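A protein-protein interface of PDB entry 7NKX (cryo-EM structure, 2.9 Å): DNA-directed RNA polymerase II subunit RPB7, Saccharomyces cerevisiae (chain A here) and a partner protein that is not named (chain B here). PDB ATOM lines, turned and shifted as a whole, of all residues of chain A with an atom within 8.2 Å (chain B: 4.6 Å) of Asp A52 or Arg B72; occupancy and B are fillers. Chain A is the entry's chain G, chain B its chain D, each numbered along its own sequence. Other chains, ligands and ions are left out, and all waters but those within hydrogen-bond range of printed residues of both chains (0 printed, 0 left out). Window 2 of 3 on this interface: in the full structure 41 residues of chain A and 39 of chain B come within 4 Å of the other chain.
The side-chain carboxylate of Asp A52 lies close to the side-chain carboxylate of Glu B65. The guanidinium group of Arg B72 lies within salt-bridge range of the side-chain carboxylate of Asp A52 (2.8 Å).
O of Ala B69 sits at hydrogen-bond distance from OG of Ser B73. The backbone carbonyl oxygen (O) of Phe B70 lies within hydrogen-bond range of the side-chain hydroxyl (OG) of Ser B73, 2.5 Å away.
Among the printed residues, merely in contact across the chains: Gln A24 with Ser B73 (3.4 Å) and Asp A52 with Ala B69 (3.5 Å).
Of the printed residues of chain B, Gln A24 touches Ser B73. Of chain B, only Glu B65, Ala B69 and Arg B72 come within 4 Å of Asp A52. Asn A53 touches none of the printed residues of chain B. Printed residues of chain A within 4 Å of Glu B65: Asp A52 (2.6 Å). Printed residues of chain A within 4 Å of Ala B69: Asp A52. Of chain A, only Asp A52 (2.8 Å) comes within 4 Å of Arg B72. Lys B76 touches none of the printed residues of chain A.
Hydrophobic or aromatic side chains of chain B within 4 Å of the printed part of chain A: Ala B69. Among the printed residues, 4 pairs touch across the chains. Among the printed residues, Asp or Glu carboxylates within 4 Å of a Lys or Arg side-chain nitrogen of the other chain: Asp A52 with Arg B72 (2.8 Å).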
ATOM      1  N   GLN A  24      13.525  14.757 -28.151  1.00  0.00           N
ATOM      2  CA  GLN A  24      14.082  14.832 -26.807  1.00  0.00           C
ATOM      3  C   GLN A  24      15.454  14.165 -26.776  1.00  0.00           C
ATOM      4  O   GLN A  24      16.373  14.626 -26.077  1.00  0.00           O
ATOM      5  CB  GLN A  24      13.105  14.177 -25.823  1.00  0.00           C
ATOM      6  CG  GLN A  24      13.612  13.897 -24.408  1.00  0.00           C
ATOM      7  CD  GLN A  24      12.566  13.194 -23.558  1.00  0.00           C
ATOM      8  OE1 GLN A  24      11.656  13.829 -23.028  1.00  0.00           O
ATOM      9  NE2 GLN A  24      12.679  11.875 -23.439  1.00  0.00           N
ATOM     10  N   LYS A  27      17.997  16.490 -28.477  1.00  0.00           N
ATOM     11  CA  LYS A  27      18.321  17.590 -27.570  1.00  0.00           C
ATOM     12  C   LYS A  27      19.304  17.163 -26.491  1.00  0.00           C
ATOM     13  O   LYS A  27      20.256  17.899 -26.209  1.00  0.00           O
ATOM     14  CB  LYS A  27      17.058  18.201 -26.955  1.00  0.00           C
ATOM     15  CG  LYS A  27      16.116  18.921 -27.923  1.00  0.00           C
ATOM     16  CD  LYS A  27      16.888  20.042 -28.616  1.00  0.00           C
ATOM     17  CE  LYS A  27      16.119  21.327 -28.765  1.00  0.00           C
ATOM     18  NZ  LYS A  27      17.148  22.392 -28.880  1.00  0.00           N
ATOM     19  N   LEU A  49      19.954  29.511 -24.906  1.00  0.00           N
ATOM     20  CA  LEU A  49      18.714  30.153 -24.482  1.00  0.00           C
ATOM     21  C   LEU A  49      17.489  29.785 -25.322  1.00  0.00           C
ATOM     22  O   LEU A  49      17.575  29.203 -26.406  1.00  0.00           O
ATOM     23  CB  LEU A  49      18.939  31.668 -24.430  1.00  0.00           C
ATOM     24  CG  LEU A  49      19.332  32.402 -25.721  1.00  0.00           C
ATOM     25  CD1 LEU A  49      18.125  32.756 -26.592  1.00  0.00           C
ATOM     26  CD2 LEU A  49      20.201  33.638 -25.430  1.00  0.00           C
ATOM     27  N   ASP A  50      16.336  30.170 -24.762  1.00  0.00           N
ATOM     28  CA  ASP A  50      14.986  30.062 -25.334  1.00  0.00           C
ATOM     29  C   ASP A  50      14.723  28.676 -25.932  1.00  0.00           C
ATOM     30  O   ASP A  50      14.427  28.518 -27.119  1.00  0.00           O
ATOM     31  CB  ASP A  50      14.763  31.167 -26.373  1.00  0.00           C
ATOM     32  CG  ASP A  50      13.296  31.393 -26.684  1.00  0.00           C
ATOM     33  OD1 ASP A  50      12.929  32.547 -26.987  1.00  0.00           O
ATOM     34  OD2 ASP A  50      12.497  30.441 -26.570  1.00  0.00           O
ATOM     35  N   TYR A  51      14.867  27.670 -25.070  1.00  0.00           N
ATOM     36  CA  TYR A  51      14.664  26.270 -25.441  1.00  0.00           C
ATOM     37  C   TYR A  51      13.345  26.001 -26.173  1.00  0.00           C
ATOM     38  O   TYR A  51      13.340  25.470 -27.290  1.00  0.00           O
ATOM     39  CB  TYR A  51      14.745  25.419 -24.175  1.00  0.00           C
ATOM     40  CG  TYR A  51      14.837  23.932 -24.408  1.00  0.00           C
ATOM     41  CD1 TYR A  51      13.690  23.155 -24.498  1.00  0.00           C
ATOM     42  CD2 TYR A  51      16.065  23.303 -24.515  1.00  0.00           C
ATOM     43  CE1 TYR A  51      13.765  21.796 -24.701  1.00  0.00           C
ATOM     44  CE2 TYR A  51      16.151  21.944 -24.717  1.00  0.00           C
ATOM     45  CZ  TYR A  51      14.998  21.196 -24.808  1.00  0.00           C
ATOM     46  OH  TYR A  51      15.084  19.839 -25.009  1.00  0.00           O
ATOM     47  N   ASP A  52      12.214  26.370 -25.554  1.00  0.00           N
ATOM     48  CA  ASP A  52      10.890  26.094 -26.128  1.00  0.00           C
ATOM     49  C   ASP A  52      10.595  26.712 -27.492  1.00  0.00           C
ATOM     50  O   ASP A  52       9.560  26.363 -28.071  1.00  0.00           O
ATOM     51  CB  ASP A  52       9.788  26.500 -25.152  1.00  0.00           C
ATOM     52  CG  ASP A  52       9.926  25.822 -23.809  1.00  0.00           C
ATOM     53  OD1 ASP A  52      10.465  26.438 -22.881  1.00  0.00           O
ATOM     54  OD2 ASP A  52       9.490  24.659 -23.686  1.00  0.00           O
ATOM     55  N   ASN A  53      11.436  27.598 -28.038  1.00  0.00           N
ATOM     56  CA  ASN A  53      11.121  28.201 -29.335  1.00  0.00           C
ATOM     57  C   ASN A  53      12.238  27.974 -30.355  1.00  0.00           C
ATOM     58  O   ASN A  53      12.235  28.588 -31.427  1.00  0.00           O
ATOM     59  CB  ASN A  53      10.843  29.698 -29.117  1.00  0.00           C
ATOM     60  CG  ASN A  53      10.391  30.460 -30.380  1.00  0.00           C
ATOM     61  OD1 ASN A  53       9.811  29.850 -31.279  1.00  0.00           O
ATOM     62  ND2 ASN A  53      10.691  31.756 -30.477  1.00  0.00           N
ATOM     63  N   ILE A  54      13.189  27.088 -30.046  1.00  0.00           N
ATOM     64  CA  ILE A  54      14.251  26.768 -30.993  1.00  0.00           C
ATOM     65  C   ILE A  54      13.663  26.246 -32.294  1.00  0.00           C
ATOM     66  O   ILE A  54      12.882  25.285 -32.297  1.00  0.00           O
ATOM     67  CB  ILE A  54      15.242  25.747 -30.419  1.00  0.00           C
ATOM     68  CG1 ILE A  54      16.287  25.437 -31.504  1.00  0.00           C
ATOM     69  CG2 ILE A  54      14.530  24.455 -29.951  1.00  0.00           C
ATOM     70  CD1 ILE A  54      17.547  24.863 -31.008  1.00  0.00           C
ATOM     71  N   ASP A  55      14.028  26.871 -33.405  1.00  0.00           N
ATOM     72  CA  ASP A  55      13.531  26.444 -34.709  1.00  0.00           C
ATOM     73  C   ASP A  55      14.449  25.306 -35.163  1.00  0.00           C
ATOM     74  O   ASP A  55      15.647  25.504 -35.376  1.00  0.00           O
ATOM     75  CB  ASP A  55      13.462  27.632 -35.671  1.00  0.00           C
ATOM     76  CG  ASP A  55      14.822  28.109 -36.152  1.00  0.00           C
ATOM     77  OD1 ASP A  55      15.432  27.449 -37.021  1.00  0.00           O
ATOM     78  OD2 ASP A  55      15.315  29.122 -35.619  1.00  0.00           O
ATOM     79  N   GLU B  65      12.548  27.595 -18.190  1.00  0.00           N
ATOM     80  CA  GLU B  65      11.850  27.115 -19.379  1.00  0.00           C
ATOM     81  C   GLU B  65      12.204  25.658 -19.684  1.00  0.00           C
ATOM     82  O   GLU B  65      11.322  24.850 -20.005  1.00  0.00           O
ATOM     83  CB  GLU B  65      12.180  28.031 -20.559  1.00  0.00           C
ATOM     84  CG  GLU B  65      11.577  29.434 -20.439  1.00  0.00           C
ATOM     85  CD  GLU B  65      10.142  29.526 -20.929  1.00  0.00           C
ATOM     86  OE1 GLU B  65       9.389  30.363 -20.391  1.00  0.00           O
ATOM     87  OE2 GLU B  65       9.764  28.777 -21.853  1.00  0.00           O
ATOM     88  N   ARG B  68      10.397  23.446 -17.198  1.00  0.00           N
ATOM     89  CA  ARG B  68       8.995  23.288 -17.574  1.00  0.00           C
ATOM     90  C   ARG B  68       8.850  22.309 -18.733  1.00  0.00           C
ATOM     91  O   ARG B  68       7.941  21.470 -18.737  1.00  0.00           O
ATOM     92  CB  ARG B  68       8.384  24.641 -17.940  1.00  0.00           C
ATOM     93  CG  ARG B  68       8.064  25.522 -16.741  1.00  0.00           C
ATOM     94  CD  ARG B  68       7.653  26.965 -17.093  1.00  0.00           C
ATOM     95  NE  ARG B  68       6.251  27.113 -17.499  1.00  0.00           N
ATOM     96  CZ  ARG B  68       5.747  26.842 -18.704  1.00  0.00           C
ATOM     97  NH1 ARG B  68       6.518  26.448 -19.710  1.00  0.00           N
ATOM     98  NH2 ARG B  68       4.450  27.018 -18.918  1.00  0.00           N
ATOM     99  N   ALA B  69       9.746  22.396 -19.722  1.00  0.00           N
ATOM    100  CA  ALA B  69       9.700  21.462 -20.843  1.00  0.00           C
ATOM    101  C   ALA B  69       9.937  20.029 -20.379  1.00  0.00           C
ATOM    102  O   ALA B  69       9.254  19.101 -20.828  1.00  0.00           O
ATOM    103  CB  ALA B  69      10.733  21.856 -21.898  1.00  0.00           C
ATOM    104  N   PHE B  70      10.905  19.828 -19.482  1.00  0.00           N
ATOM    105  CA  PHE B  70      11.197  18.485 -18.991  1.00  0.00           C
ATOM    106  C   PHE B  70      10.019  17.922 -18.204  1.00  0.00           C
ATOM    107  O   PHE B  70       9.661  16.743 -18.352  1.00  0.00           O
ATOM    108  CB  PHE B  70      12.456  18.505 -18.124  1.00  0.00           C
ATOM    109  CG  PHE B  70      13.278  17.255 -18.225  1.00  0.00           C
ATOM    110  CD1 PHE B  70      13.193  16.271 -17.253  1.00  0.00           C
ATOM    111  CD2 PHE B  70      14.140  17.065 -19.291  1.00  0.00           C
ATOM    112  CE1 PHE B  70      13.950  15.119 -17.346  1.00  0.00           C
ATOM    113  CE2 PHE B  70      14.900  15.916 -19.391  1.00  0.00           C
ATOM    114  CZ  PHE B  70      14.806  14.941 -18.416  1.00  0.00           C
ATOM    115  N   LYS B  71       9.407  18.755 -17.359  1.00  0.00           N
ATOM    116  CA  LYS B  71       8.236  18.328 -16.604  1.00  0.00           C
ATOM    117  C   LYS B  71       7.096  17.953 -17.541  1.00  0.00           C
ATOM    118  O   LYS B  71       6.434  16.929 -17.341  1.00  0.00           O
ATOM    119  CB  LYS B  71       7.798  19.441 -15.650  1.00  0.00           C
ATOM    120  CG  LYS B  71       8.515  19.453 -14.300  1.00  0.00           C
ATOM    121  CD  LYS B  71       7.623  19.956 -13.168  1.00  0.00           C
ATOM    122  CE  LYS B  71       7.312  21.446 -13.291  1.00  0.00           C
ATOM    123  NZ  LYS B  71       8.457  22.294 -12.864  1.00  0.00           N
ATOM    124  N   ARG B  72       6.865  18.763 -18.578  1.00  0.00           N
ATOM    125  CA  ARG B  72       5.818  18.453 -19.547  1.00  0.00           C
ATOM    126  C   ARG B  72       6.110  17.134 -20.254  1.00  0.00           C
ATOM    127  O   ARG B  72       5.203  16.322 -20.467  1.00  0.00           O
ATOM    128  CB  ARG B  72       5.695  19.603 -20.554  1.00  0.00           C
ATOM    129  CG  ARG B  72       4.726  19.400 -21.743  1.00  0.00           C
ATOM    130  CD  ARG B  72       5.306  19.928 -23.051  1.00  0.00           C
ATOM    131  NE  ARG B  72       5.828  21.290 -22.922  1.00  0.00           N
ATOM    132  CZ  ARG B  72       6.829  21.808 -23.633  1.00  0.00           C
ATOM    133  NH1 ARG B  72       7.458  21.105 -24.571  1.00  0.00           N
ATOM    134  NH2 ARG B  72       7.202  23.060 -23.409  1.00  0.00           N
ATOM    135  N   SER B  73       7.371  16.909 -20.634  1.00  0.00           N
ATOM    136  CA  SER B  73       7.719  15.686 -21.350  1.00  0.00           C
ATOM    137  C   SER B  73       7.473  14.457 -20.488  1.00  0.00           C
ATOM    138  O   SER B  73       6.884  13.473 -20.953  1.00  0.00           O
ATOM    139  CB  SER B  73       9.180  15.727 -21.794  1.00  0.00           C
ATOM    140  OG  SER B  73      10.012  16.163 -20.738  1.00  0.00           O
ATOM    141  N   GLN B  74       7.912  14.491 -19.226  1.00  0.00           N
ATOM    142  CA  GLN B  74       7.754  13.309 -18.382  1.00  0.00           C
ATOM    143  C   GLN B  74       6.321  13.203 -17.861  1.00  0.00           C
ATOM    144  O   GLN B  74       5.923  12.152 -17.351  1.00  0.00           O
ATOM    145  CB  GLN B  74       8.764  13.359 -17.231  1.00  0.00           C
ATOM    146  CG  GLN B  74       8.672  12.268 -16.140  1.00  0.00           C
ATOM    147  CD  GLN B  74       8.471  10.853 -16.685  1.00  0.00           C
ATOM    148  OE1 GLN B  74       7.411  10.249 -16.528  1.00  0.00           O
ATOM    149  NE2 GLN B  74       9.496  10.329 -17.344  1.00  0.00           N
ATOM    150  N   LYS B  75       5.518  14.265 -17.991  1.00  0.00           N
ATOM    151  CA  LYS B  75       4.105  14.154 -17.647  1.00  0.00           C
ATOM    152  C   LYS B  75       3.409  13.121 -18.524  1.00  0.00           C
ATOM    153  O   LYS B  75       2.650  12.282 -18.024  1.00  0.00           O
ATOM    154  CB  LYS B  75       3.424  15.518 -17.774  1.00  0.00           C
ATOM    155  CG  LYS B  75       2.170  15.667 -16.921  1.00  0.00           C
ATOM    156  CD  LYS B  75       1.638  17.103 -16.939  1.00  0.00           C
ATOM    157  CE  LYS B  75       0.733  17.417 -15.745  1.00  0.00           C
ATOM    158  NZ  LYS B  75       0.923  18.808 -15.247  1.00  0.00           N
ATOM    159  N   LYS B  76       3.662  13.159 -19.829  1.00  0.00           N
ATOM    160  CA  LYS B  76       3.182  12.124 -20.738  1.00  0.00           C
ATOM    161  C   LYS B  76       3.885  12.221 -22.088  1.00  0.00           C
ATOM    162  O   LYS B  76       3.551  13.072 -22.913  1.00  0.00           O
ATOM    163  CB  LYS B  76       1.661  12.223 -20.931  1.00  0.00           C
ATOM    164  CG  LYS B  76       0.988  11.127 -21.795  1.00  0.00           C
ATOM    165  CD  LYS B  76       1.467   9.682 -21.561  1.00  0.00           C
ATOM    166  CE  LYS B  76       0.800   9.066 -20.342  1.00  0.00           C
ATOM    167  NZ  LYS B  76       1.599   7.944 -19.777  1.00  0.00           N
